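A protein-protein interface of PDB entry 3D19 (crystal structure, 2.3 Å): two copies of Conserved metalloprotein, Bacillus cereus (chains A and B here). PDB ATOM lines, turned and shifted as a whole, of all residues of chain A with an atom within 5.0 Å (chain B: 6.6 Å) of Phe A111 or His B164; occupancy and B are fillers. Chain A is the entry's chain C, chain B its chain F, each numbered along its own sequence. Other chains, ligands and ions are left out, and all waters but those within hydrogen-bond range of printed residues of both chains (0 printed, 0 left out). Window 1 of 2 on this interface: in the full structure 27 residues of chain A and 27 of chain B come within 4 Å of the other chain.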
ATOM      1  N   GLN A 108     -24.168  14.773  -5.551  1.00  0.00           N
ATOM      2  CA  GLN A 108     -24.178  15.938  -4.636  1.00  0.00           C
ATOM      3  C   GLN A 108     -24.368  15.534  -3.171  1.00  0.00           C
ATOM      4  O   GLN A 108     -24.880  14.459  -2.889  1.00  0.00           O
ATOM      5  CB  GLN A 108     -25.260  16.945  -5.053  1.00  0.00           C
ATOM      6  CG  GLN A 108     -26.654  16.475  -4.769  1.00  0.00           C
ATOM      7  CD  GLN A 108     -27.136  16.981  -3.443  1.00  0.00           C
ATOM      8  OE1 GLN A 108     -26.806  18.106  -3.059  1.00  0.00           O
ATOM      9  NE2 GLN A 108     -27.936  16.168  -2.727  1.00  0.00           N
ATOM     10  N   ASN A 109     -23.973  16.384  -2.241  1.00  0.00           N
ATOM     11  CA  ASN A 109     -24.031  16.005  -0.863  1.00  0.00           C
ATOM     12  C   ASN A 109     -24.807  16.951   0.034  1.00  0.00           C
ATOM     13  O   ASN A 109     -24.589  16.947   1.260  1.00  0.00           O
ATOM     14  CB  ASN A 109     -22.624  15.871  -0.304  1.00  0.00           C
ATOM     15  CG  ASN A 109     -21.784  14.910  -1.082  1.00  0.00           C
ATOM     16  OD1 ASN A 109     -22.024  13.684  -1.046  1.00  0.00           O
ATOM     17  ND2 ASN A 109     -20.759  15.441  -1.803  1.00  0.00           N
ATOM     18  N   ASN A 110     -25.684  17.768  -0.541  1.00  0.00           N
ATOM     19  CA  ASN A 110     -26.609  18.518   0.285  1.00  0.00           C
ATOM     20  C   ASN A 110     -27.895  17.726   0.537  1.00  0.00           C
ATOM     21  O   ASN A 110     -28.624  17.445  -0.393  1.00  0.00           O
ATOM     22  CB  ASN A 110     -26.986  19.847  -0.367  1.00  0.00           C
ATOM     23  CG  ASN A 110     -25.834  20.797  -0.449  1.00  0.00           C
ATOM     24  OD1 ASN A 110     -25.130  21.012   0.531  1.00  0.00           O
ATOM     25  ND2 ASN A 110     -25.637  21.391  -1.614  1.00  0.00           N
ATOM     26  N   PHE A 111     -28.160  17.372   1.786  1.00  0.00           N
ATOM     27  CA  PHE A 111     -29.456  16.808   2.174  1.00  0.00           C
ATOM     28  C   PHE A 111     -30.603  17.725   1.700  1.00  0.00           C
ATOM     29  O   PHE A 111     -30.578  18.889   1.976  1.00  0.00           O
ATOM     30  CB  PHE A 111     -29.525  16.685   3.716  1.00  0.00           C
ATOM     31  CG  PHE A 111     -28.738  15.527   4.279  1.00  0.00           C
ATOM     32  CD1 PHE A 111     -28.961  14.235   3.822  1.00  0.00           C
ATOM     33  CD2 PHE A 111     -27.810  15.716   5.283  1.00  0.00           C
ATOM     34  CE1 PHE A 111     -28.269  13.166   4.328  1.00  0.00           C
ATOM     35  CE2 PHE A 111     -27.116  14.639   5.837  1.00  0.00           C
ATOM     36  CZ  PHE A 111     -27.351  13.337   5.326  1.00  0.00           C
ATOM     37  N   PRO A 112     -31.591  17.185   0.966  1.00  0.00           N
ATOM     38  CA  PRO A 112     -32.793  17.993   0.672  1.00  0.00           C
ATOM     39  C   PRO A 112     -33.417  18.651   1.919  1.00  0.00           C
ATOM     40  O   PRO A 112     -33.912  19.820   1.818  1.00  0.00           O
ATOM     41  CB  PRO A 112     -33.778  16.997   0.082  1.00  0.00           C
ATOM     42  CG  PRO A 112     -32.947  15.769  -0.331  1.00  0.00           C
ATOM     43  CD  PRO A 112     -31.721  15.775   0.539  1.00  0.00           C
ATOM     44  N   LEU A 113     -33.382  17.942   3.064  1.00  0.00           N
ATOM     45  CA  LEU A 113     -33.960  18.436   4.315  1.00  0.00           C
ATOM     46  C   LEU A 113     -33.222  19.674   4.838  1.00  0.00           C
ATOM     47  O   LEU A 113     -33.796  20.678   5.339  1.00  0.00           O
ATOM     48  CB  LEU A 113     -33.963  17.328   5.381  1.00  0.00           C
ATOM     49  CG  LEU A 113     -34.587  17.648   6.764  1.00  0.00           C
ATOM     50  CD1 LEU A 113     -35.667  18.825   6.715  1.00  0.00           C
ATOM     51  CD2 LEU A 113     -35.213  16.377   7.401  1.00  0.00           C
ATOM     52  N   LEU A 114     -31.924  19.605   4.681  1.00  0.00           N
ATOM     53  CA  LEU A 114     -31.080  20.711   4.998  1.00  0.00           C
ATOM     54  C   LEU A 114     -31.370  21.867   4.047  1.00  0.00           C
ATOM     55  O   LEU A 114     -31.532  23.005   4.496  1.00  0.00           O
ATOM     56  CB  LEU A 114     -29.619  20.242   4.946  1.00  0.00           C
ATOM     57  CG  LEU A 114     -28.638  21.282   5.492  1.00  0.00           C
ATOM     58  CD1 LEU A 114     -27.380  20.631   6.142  1.00  0.00           C
ATOM     59  CD2 LEU A 114     -28.241  22.219   4.367  1.00  0.00           C
ATOM     60  N   VAL A 115     -31.453  21.618   2.727  1.00  0.00           N
ATOM     61  CA  VAL A 115     -31.817  22.738   1.812  1.00  0.00           C
ATOM     62  C   VAL A 115     -33.187  23.361   2.168  1.00  0.00           C
ATOM     63  O   VAL A 115     -33.329  24.596   2.238  1.00  0.00           O
ATOM     64  CB  VAL A 115     -31.760  22.357   0.304  1.00  0.00           C
ATOM     65  CG1 VAL A 115     -32.218  23.529  -0.594  1.00  0.00           C
ATOM     66  CG2 VAL A 115     -30.348  21.919  -0.085  1.00  0.00           C
ATOM     67  N   PHE A 161     -29.412  16.372  11.486  1.00  0.00           N
ATOM     68  CA  PHE A 161     -28.192  16.680  10.714  1.00  0.00           C
ATOM     69  C   PHE A 161     -26.920  16.228  11.513  1.00  0.00           C
ATOM     70  O   PHE A 161     -25.984  15.582  10.985  1.00  0.00           O
ATOM     71  CB  PHE A 161     -28.038  18.189  10.378  1.00  0.00           C
ATOM     72  CG  PHE A 161     -29.228  18.858   9.699  1.00  0.00           C
ATOM     73  CD1 PHE A 161     -30.030  18.203   8.783  1.00  0.00           C
ATOM     74  CD2 PHE A 161     -29.492  20.221   9.969  1.00  0.00           C
ATOM     75  CE1 PHE A 161     -31.127  18.862   8.153  1.00  0.00           C
ATOM     76  CE2 PHE A 161     -30.567  20.890   9.367  1.00  0.00           C
ATOM     77  CZ  PHE A 161     -31.386  20.198   8.445  1.00  0.00           C
ATOM     78  N   GLY A 163     -26.625  13.928  13.875  1.00  0.00           N
ATOM     79  CA  GLY A 163     -26.575  12.485  13.928  1.00  0.00           C
ATOM     80  C   GLY A 163     -26.183  11.802  12.641  1.00  0.00           C
ATOM     81  O   GLY A 163     -25.604  10.727  12.692  1.00  0.00           O
ATOM     82  N   HIS A 164     -26.492  12.427  11.507  1.00  0.00           N
ATOM     83  CA  HIS A 164     -26.198  11.912  10.165  1.00  0.00           C
ATOM     84  C   HIS A 164     -24.780  12.229   9.734  1.00  0.00           C
ATOM     85  O   HIS A 164     -24.075  11.367   9.157  1.00  0.00           O
ATOM     86  CB  HIS A 164     -27.162  12.506   9.129  1.00  0.00           C
ATOM     87  CG  HIS A 164     -28.471  11.779   9.039  1.00  0.00           C
ATOM     88  ND1 HIS A 164     -28.875  11.112   7.905  1.00  0.00           N
ATOM     89  CD2 HIS A 164     -29.445  11.585   9.947  1.00  0.00           C
ATOM     90  CE1 HIS A 164     -30.053  10.552   8.110  1.00  0.00           C
ATOM     91  NE2 HIS A 164     -30.432  10.835   9.340  1.00  0.00           N
ATOM     92  N   LEU A 165     -24.376  13.474   9.977  1.00  0.00           N
ATOM     93  CA  LEU A 165     -23.054  13.937   9.642  1.00  0.00           C
ATOM     94  C   LEU A 165     -21.959  13.371  10.578  1.00  0.00           C
ATOM     95  O   LEU A 165     -20.781  13.380  10.246  1.00  0.00           O
ATOM     96  CB  LEU A 165     -23.047  15.446   9.630  1.00  0.00           C
ATOM     97  CG  LEU A 165     -23.434  16.132   8.292  1.00  0.00           C
ATOM     98  CD1 LEU A 165     -23.975  15.138   7.290  1.00  0.00           C
ATOM     99  CD2 LEU A 165     -24.341  17.402   8.403  1.00  0.00           C
ATOM    100  N   LEU A 166     -22.335  12.835  11.725  1.00  0.00           N
ATOM    101  CA  LEU A 166     -21.373  12.146  12.578  1.00  0.00           C
ATOM    102  C   LEU A 166     -20.888  10.843  11.897  1.00  0.00           C
ATOM    103  O   LEU A 166     -21.673  10.092  11.253  1.00  0.00           O
ATOM    104  CB  LEU A 166     -21.996  11.825  13.931  1.00  0.00           C
ATOM    105  CG  LEU A 166     -21.969  12.846  15.076  1.00  0.00           C
ATOM    106  CD1 LEU A 166     -22.854  12.360  16.173  1.00  0.00           C
ATOM    107  CD2 LEU A 166     -20.582  13.047  15.638  1.00  0.00           C
ATOM    108  N   ASP A 167     -19.608  10.544  12.037  1.00  0.00           N
ATOM    109  CA  ASP A 167     -19.161   9.275  11.529  1.00  0.00           C
ATOM    110  C   ASP A 167     -19.982   8.231  12.221  1.00  0.00           C
ATOM    111  O   ASP A 167     -20.197   8.310  13.413  1.00  0.00           O
ATOM    112  CB  ASP A 167     -17.672   9.053  11.773  1.00  0.00           C
ATOM    113  CG  ASP A 167     -17.191   7.725  11.153  1.00  0.00           C
ATOM    114  OD1 ASP A 167     -17.243   7.609   9.920  1.00  0.00           O
ATOM    115  OD2 ASP A 167     -16.799   6.784  11.889  1.00  0.00           O
ATOM    116  N   PRO A 168     -20.455   7.238  11.468  1.00  0.00           N
ATOM    117  CA  PRO A 168     -21.220   6.124  12.010  1.00  0.00           C
ATOM    118  C   PRO A 168     -20.542   5.398  13.155  1.00  0.00           C
ATOM    119  O   PRO A 168     -21.206   4.689  13.927  1.00  0.00           O
ATOM    120  CB  PRO A 168     -21.333   5.172  10.812  1.00  0.00           C
ATOM    121  CG  PRO A 168     -21.282   6.011   9.634  1.00  0.00           C
ATOM    122  CD  PRO A 168     -20.578   7.317  10.006  1.00  0.00           C
ATOM    123  N   VAL A 174     -23.763   9.568  18.175  1.00  0.00           N
ATOM    124  CA  VAL A 174     -24.896   9.293  17.326  1.00  0.00           C
ATOM    125  C   VAL A 174     -26.144   9.012  18.150  1.00  0.00           C
ATOM    126  O   VAL A 174     -27.232   9.568  17.874  1.00  0.00           O
ATOM    127  CB  VAL A 174     -24.667   8.084  16.325  1.00  0.00           C
ATOM    128  CG1 VAL A 174     -26.057   7.603  15.779  1.00  0.00           C
ATOM    129  CG2 VAL A 174     -23.661   8.452  15.154  1.00  0.00           C
ATOM    130  N   PHE B 111     -16.829   9.933   4.860  1.00  0.00           N
ATOM    131  CA  PHE B 111     -16.878   9.382   6.203  1.00  0.00           C
ATOM    132  C   PHE B 111     -15.588   8.600   6.509  1.00  0.00           C
ATOM    133  O   PHE B 111     -15.266   7.638   5.784  1.00  0.00           O
ATOM    134  CB  PHE B 111     -18.053   8.412   6.369  1.00  0.00           C
ATOM    135  CG  PHE B 111     -19.364   9.077   6.690  1.00  0.00           C
ATOM    136  CD1 PHE B 111     -19.448  10.004   7.720  1.00  0.00           C
ATOM    137  CD2 PHE B 111     -20.534   8.728   5.997  1.00  0.00           C
ATOM    138  CE1 PHE B 111     -20.620  10.594   8.042  1.00  0.00           C
ATOM    139  CE2 PHE B 111     -21.743   9.330   6.317  1.00  0.00           C
ATOM    140  CZ  PHE B 111     -21.773  10.274   7.349  1.00  0.00           C
ATOM    141  N   ALA B 159     -25.371  -0.915   6.353  1.00  0.00           N
ATOM    142  CA  ALA B 159     -26.597  -0.556   7.000  1.00  0.00           C
ATOM    143  C   ALA B 159     -26.500   0.852   7.597  1.00  0.00           C
ATOM    144  O   ALA B 159     -27.453   1.607   7.474  1.00  0.00           O
ATOM    145  CB  ALA B 159     -26.911  -1.566   8.077  1.00  0.00           C
ATOM    146  N   LYS B 160     -25.368   1.202   8.218  1.00  0.00           N
ATOM    147  CA  LYS B 160     -25.104   2.600   8.687  1.00  0.00           C
ATOM    148  C   LYS B 160     -24.833   3.623   7.562  1.00  0.00           C
ATOM    149  O   LYS B 160     -25.220   4.811   7.667  1.00  0.00           O
ATOM    150  CB  LYS B 160     -23.929   2.649   9.694  1.00  0.00           C
ATOM    151  CG  LYS B 160     -24.249   1.947  10.991  1.00  0.00           C
ATOM    152  CD  LYS B 160     -23.020   1.809  11.796  1.00  0.00           C
ATOM    153  CE  LYS B 160     -23.219   0.820  12.929  1.00  0.00           C
ATOM    154  NZ  LYS B 160     -23.219  -0.586  12.469  1.00  0.00           N
ATOM    155  N   PHE B 161     -24.127   3.217   6.510  1.00  0.00           N
ATOM    156  CA  PHE B 161     -23.916   4.198   5.432  1.00  0.00           C
ATOM    157  C   PHE B 161     -25.249   4.633   4.859  1.00  0.00           C
ATOM    158  O   PHE B 161     -25.512   5.824   4.709  1.00  0.00           O
ATOM    159  CB  PHE B 161     -22.980   3.694   4.324  1.00  0.00           C
ATOM    160  CG  PHE B 161     -21.613   3.335   4.831  1.00  0.00           C
ATOM    161  CD1 PHE B 161     -21.023   4.101   5.846  1.00  0.00           C
ATOM    162  CD2 PHE B 161     -20.916   2.235   4.302  1.00  0.00           C
ATOM    163  CE1 PHE B 161     -19.756   3.753   6.341  1.00  0.00           C
ATOM    164  CE2 PHE B 161     -19.663   1.891   4.797  1.00  0.00           C
ATOM    165  CZ  PHE B 161     -19.087   2.652   5.812  1.00  0.00           C
ATOM    166  N   ILE B 162     -26.115   3.659   4.583  1.00  0.00           N
ATOM    167  CA  ILE B 162     -27.434   3.950   4.048  1.00  0.00           C
ATOM    168  C   ILE B 162     -28.278   4.851   4.956  1.00  0.00           C
ATOM    169  O   ILE B 162     -28.951   5.758   4.474  1.00  0.00           O
ATOM    170  CB  ILE B 162     -28.186   2.683   3.873  1.00  0.00           C
ATOM    171  CG1 ILE B 162     -27.625   1.905   2.690  1.00  0.00           C
ATOM    172  CG2 ILE B 162     -29.683   2.918   3.733  1.00  0.00           C
ATOM    173  CD1 ILE B 162     -27.861   0.489   2.919  1.00  0.00           C
ATOM    174  N   GLY B 163     -28.307   4.516   6.230  1.00  0.00           N
ATOM    175  CA  GLY B 163     -29.121   5.250   7.174  1.00  0.00           C
ATOM    176  C   GLY B 163     -28.564   6.642   7.326  1.00  0.00           C
ATOM    177  O   GLY B 163     -29.298   7.550   7.444  1.00  0.00           O
ATOM    178  N   HIS B 164     -27.244   6.800   7.291  1.00  0.00           N
ATOM    179  CA  HIS B 164     -26.644   8.130   7.338  1.00  0.00           C
ATOM    180  C   HIS B 164     -26.849   8.942   6.051  1.00  0.00           C
ATOM    181  O   HIS B 164     -27.084  10.162   6.116  1.00  0.00           O
ATOM    182  CB  HIS B 164     -25.162   8.057   7.756  1.00  0.00           C
ATOM    183  CG  HIS B 164     -24.961   7.844   9.231  1.00  0.00           C
ATOM    184  ND1 HIS B 164     -24.447   8.818  10.065  1.00  0.00           N
ATOM    185  CD2 HIS B 164     -25.236   6.786  10.027  1.00  0.00           C
ATOM    186  CE1 HIS B 164     -24.408   8.368  11.307  1.00  0.00           C
ATOM    187  NE2 HIS B 164     -24.880   7.136  11.312  1.00  0.00           N
ATOM    188  N   LEU B 165     -26.799   8.296   4.885  1.00  0.00           N
ATOM    189  CA  LEU B 165     -26.967   9.026   3.614  1.00  0.00           C
ATOM    190  C   LEU B 165     -28.424   9.155   3.151  1.00  0.00           C
ATOM    191  O   LEU B 165     -28.711   9.785   2.153  1.00  0.00           O
ATOM    192  CB  LEU B 165     -26.130   8.418   2.494  1.00  0.00           C
ATOM    193  CG  LEU B 165     -24.615   8.664   2.390  1.00  0.00           C
ATOM    194  CD1 LEU B 165     -24.042   9.853   3.238  1.00  0.00           C
ATOM    195  CD2 LEU B 165     -23.791   7.386   2.555  1.00  0.00           C
ATOM    196  N   LEU B 166     -29.346   8.549   3.863  1.00  0.00           N
ATOM    197  CA  LEU B 166     -30.749   8.742   3.544  1.00  0.00           C
ATOM    198  C   LEU B 166     -31.042  10.190   4.031  1.00  0.00           C
ATOM    199  O   LEU B 166     -30.375  10.693   4.942  1.00  0.00           O
ATOM    200  CB  LEU B 166     -31.586   7.711   4.279  1.00  0.00           C
ATOM    201  CG  LEU B 166     -31.855   6.378   3.517  1.00  0.00           C
ATOM    202  CD1 LEU B 166     -32.417   5.300   4.415  1.00  0.00           C
ATOM    203  CD2 LEU B 166     -32.841   6.613   2.381  1.00  0.00           C
ATOM    204  N   ASP B 167     -31.943  10.885   3.364  1.00  0.00           N
ATOM    205  CA  ASP B 167     -32.369  12.175   3.881  1.00  0.00           C
ATOM    206  C   ASP B 167     -33.023  11.899   5.240  1.00  0.00           C
ATOM    207  O   ASP B 167     -33.789  10.955   5.365  1.00  0.00           O
ATOM    208  CB  ASP B 167     -33.368  12.829   2.959  1.00  0.00           C
ATOM    209  CG  ASP B 167     -33.660  14.246   3.373  1.00  0.00           C
ATOM    210  OD1 ASP B 167     -32.714  15.056   3.313  1.00  0.00           O
ATOM    211  OD2 ASP B 167     -34.819  14.551   3.760  1.00  0.00           O
ATOM    212  N   PRO B 168     -32.723  12.728   6.266  1.00  0.00           N
ATOM    213  CA  PRO B 168     -33.463  12.618   7.557  1.00  0.00           C
ATOM    214  C   PRO B 168     -35.009  12.729   7.496  1.00  0.00           C
ATOM    215  O   PRO B 168     -35.676  12.252   8.451  1.00  0.00           O
ATOM    216  CB  PRO B 168     -32.888  13.758   8.407  1.00  0.00           C
ATOM    217  CG  PRO B 168     -31.590  14.217   7.722  1.00  0.00           C
ATOM    218  CD  PRO B 168     -31.706  13.805   6.270  1.00  0.00           C
ATOM    219  N   VAL B 174     -34.931   5.257   7.258  1.00  0.00           N
ATOM    220  CA  VAL B 174     -33.821   5.537   8.181  1.00  0.00           C
ATOM    221  C   VAL B 174     -33.947   4.561   9.354  1.00  0.00           C
ATOM    222  O   VAL B 174     -33.001   3.879   9.754  1.00  0.00           O
ATOM    223  CB  VAL B 174     -33.888   7.053   8.754  1.00  0.00           C
ATOM    224  CG1 VAL B 174     -33.087   7.185  10.063  1.00  0.00           C
ATOM    225  CG2 VAL B 174     -33.434   8.121   7.730  1.00  0.00           C
ATOM    226  N   ALA B 177     -33.180   0.860   8.163  1.00  0.00           N
ATOM    227  CA  ALA B 177     -31.733   0.630   8.040  1.00  0.00           C
ATOM    228  C   ALA B 177     -31.106   0.556   9.417  1.00  0.00           C
ATOM    229  O   ALA B 177     -30.114  -0.154   9.618  1.00  0.00           O
ATOM    230  CB  ALA B 177     -31.057   1.726   7.231  1.00  0.00           C
ATOM    231  N   SER B 239     -32.336  11.290  -0.637  1.00  0.00           N
ATOM    232  CA  SER B 239     -31.148  10.649  -0.190  1.00  0.00           C
ATOM    233  C   SER B 239     -29.988  11.392  -0.800  1.00  0.00           C
ATOM    234  O   SER B 239     -30.133  12.039  -1.821  1.00  0.00           O
ATOM    235  CB  SER B 239     -31.128   9.163  -0.690  1.00  0.00           C
ATOM    236  OG  SER B 239     -30.363   9.045  -1.898  1.00  0.00           O
ATOM    237  N   ILE B 240     -28.813  11.297  -0.208  1.00  0.00           N
ATOM    238  CA  ILE B 240     -27.641  11.685  -0.983  1.00  0.00           C
ATOM    239  C   ILE B 240     -26.915  10.401  -1.406  1.00  0.00           C
ATOM    240  O   ILE B 240     -25.707  10.375  -1.489  1.00  0.00           O
ATOM    241  CB  ILE B 240     -26.734  12.722  -0.294  1.00  0.00           C
ATOM    242  CG1 ILE B 240     -26.112  12.160   0.970  1.00  0.00           C
ATOM    243  CG2 ILE B 240     -27.532  14.050   0.005  1.00  0.00           C
ATOM    244  CD1 ILE B 240     -25.532  13.218   1.865  1.00  0.00           C
ATOM    245  N   ILE B 241     -27.668   9.332  -1.672  1.00  0.00           N
ATOM    246  CA  ILE B 241     -27.032   8.056  -2.056  1.00  0.00           C
ATOM    247  C   ILE B 241     -26.954   7.981  -3.576  1.00  0.00           C
ATOM    248  O   ILE B 241     -27.987   7.920  -4.230  1.00  0.00           O
ATOM    249  CB  ILE B 241     -27.769   6.842  -1.493  1.00  0.00           C
ATOM    250  CG1 ILE B 241     -27.631   6.812   0.055  1.00  0.00           C
ATOM    251  CG2 ILE B 241     -27.225   5.496  -2.133  1.00  0.00           C
ATOM    252  CD1 ILE B 241     -28.799   6.145   0.794  1.00  0.00           C
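The backbone carbonyl oxygen (O) of His B164 is in hydrogen-bond range of a ring nitrogen (ND1) of His A164.
The backbone NH (N) of Leu A113 is in hydrogen-bond range of the side-chain carboxylate (OD1) of Asp B167, 3.0 Å away.
The backbone carbonyl oxygen (O) of Leu B166 lies close to a ring nitrogen (ND1) of His A164.
The side-chain carboxylate of Asp B167 sits close to the backbone nitrogen of Pro A112, 3.4 Å away.
O of Gly A163 sits close to ND1 of His B164, at 3.4 Å.
O of Leu A166 sits close to ND1 of His B164 (3.3 Å).
The backbone carbonyl oxygen of Asn A110 sits at hydrogen-bond distance from the side-chain amide nitrogen of Gln A108, 2.7 Å away.
O of Leu B165 is in hydrogen-bond range of N of Ile B240 (2.8 Å).
Among the printed residues, merely in contact across the chains: Gln A108 with Ile B240 (3.5 Å), Asn A109 with Ile B240 (3.9 Å), Asn A110 with Ile B240 (3.6 Å), Phe A111 with His B164 (3.3 Å), Phe A111 with Leu B166 (3.3 Å), Phe A111 with Asp B167 (3.6 Å), Phe A111 with Pro B168 (3.7 Å), Phe A111 with Ile B240 (3.7 Å), Leu A113 with Pro B168 (3.6 Å), His A164 with Phe B111 (3.1 Å), His A164 with Gly B163 (3.2 Å), His A164 with Pro B168 (3.9 Å), Leu A165 with Phe B111 (3.6 Å), Leu A166 with Phe B111 (3.4 Å), Asp A167 with Phe B111 (3.7 Å), Pro A168 with Phe B111 (3.7 Å), Pro A168 with Lys B160 (3.8 Å), Pro A168 with His B164 (3.9 Å) and Val A174 with His B164 (3.9 Å).
Of the printed residues of chain B, Asn A109 touches Ile B240 (3.9 Å).
Of chain B, only His B164, Leu B166, Asp B167, Pro B168 and Ile B240 come within 4 Å of Phe A111.
Val A115 touches none of the printed residues of chain B.
Of the printed residues of chain B, His A164 touches Phe B111 (3.1 Å), Gly B163 (3.2 Å), His B164 (2.7 Å), Leu B166 (3.2 Å) and Pro B168 (3.9 Å).
Of the printed residues of chain B, Pro A168 touches Phe B111 (3.7 Å), Lys B160 (3.8 Å) and His B164 (3.9 Å).
Printed residues of chain A within 4 Å of Phe B111: His A164, Leu A165, Leu A166, Asp A167 and Pro A168.
Ala B159 touches none of the printed residues of chain A.
Printed residues of chain A within 4 Å of His B164: Phe A111, Gly A163, His A164, Leu A166, Pro A168 and Val A174.
Printed residues of chain A within 4 Å of Pro B168: Phe A111 (3.7 Å), Leu A113 (3.6 Å) and His A164 (3.9 Å).
The nearest residue of chain B that does not touch Phe A111 is Leu B165 (4.04 Å).
The nearest residue of chain A that does not touch His B164 is Asp A167 (4.5 Å).
The nearest printed residue of chain B that does not touch Asp A167 is His B164 (4.5 Å).
Printed residues of chain A that touch a printed residue of chain B: Gln A108, Asn A109, Asn A110, Phe A111, Pro A112, Leu A113, Gly A163, His A164, Leu A165, Leu A166, Asp A167, Pro A168 and Val A174.
Hydrophobic or aromatic side chains of chain A within 4 Å of the printed part of chain B: Phe A111, Pro A112, Leu A113, His A164, Pro A168 and Val A174.
Of the 16 printed residues of chain B, 8 touch a printed residue of chain A.
Among the printed residues, 25 pairs touch across the chains.
Among the printed residues, no Asp or Glu carboxylate lies within 4 Å of a Lys or Arg side-chain nitrogen of the other chain.
Phe A111 touches His B164, and with the chains exchanged His A164 touches Phe B111.
Phe A111 touches Asp B167, and with the chains exchanged Asp A167 touches Phe B111.
His A164 touches Pro B168, and with the chains exchanged Pro A168 touches His B164.
Leu A165 touches Phe B111, but with the chains exchanged Phe A111 does not touch Leu B165 (4.04 Å).
Positions printed for both chains: 111, 161, 163, 164, 165, 166, 167, 168 and 174.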
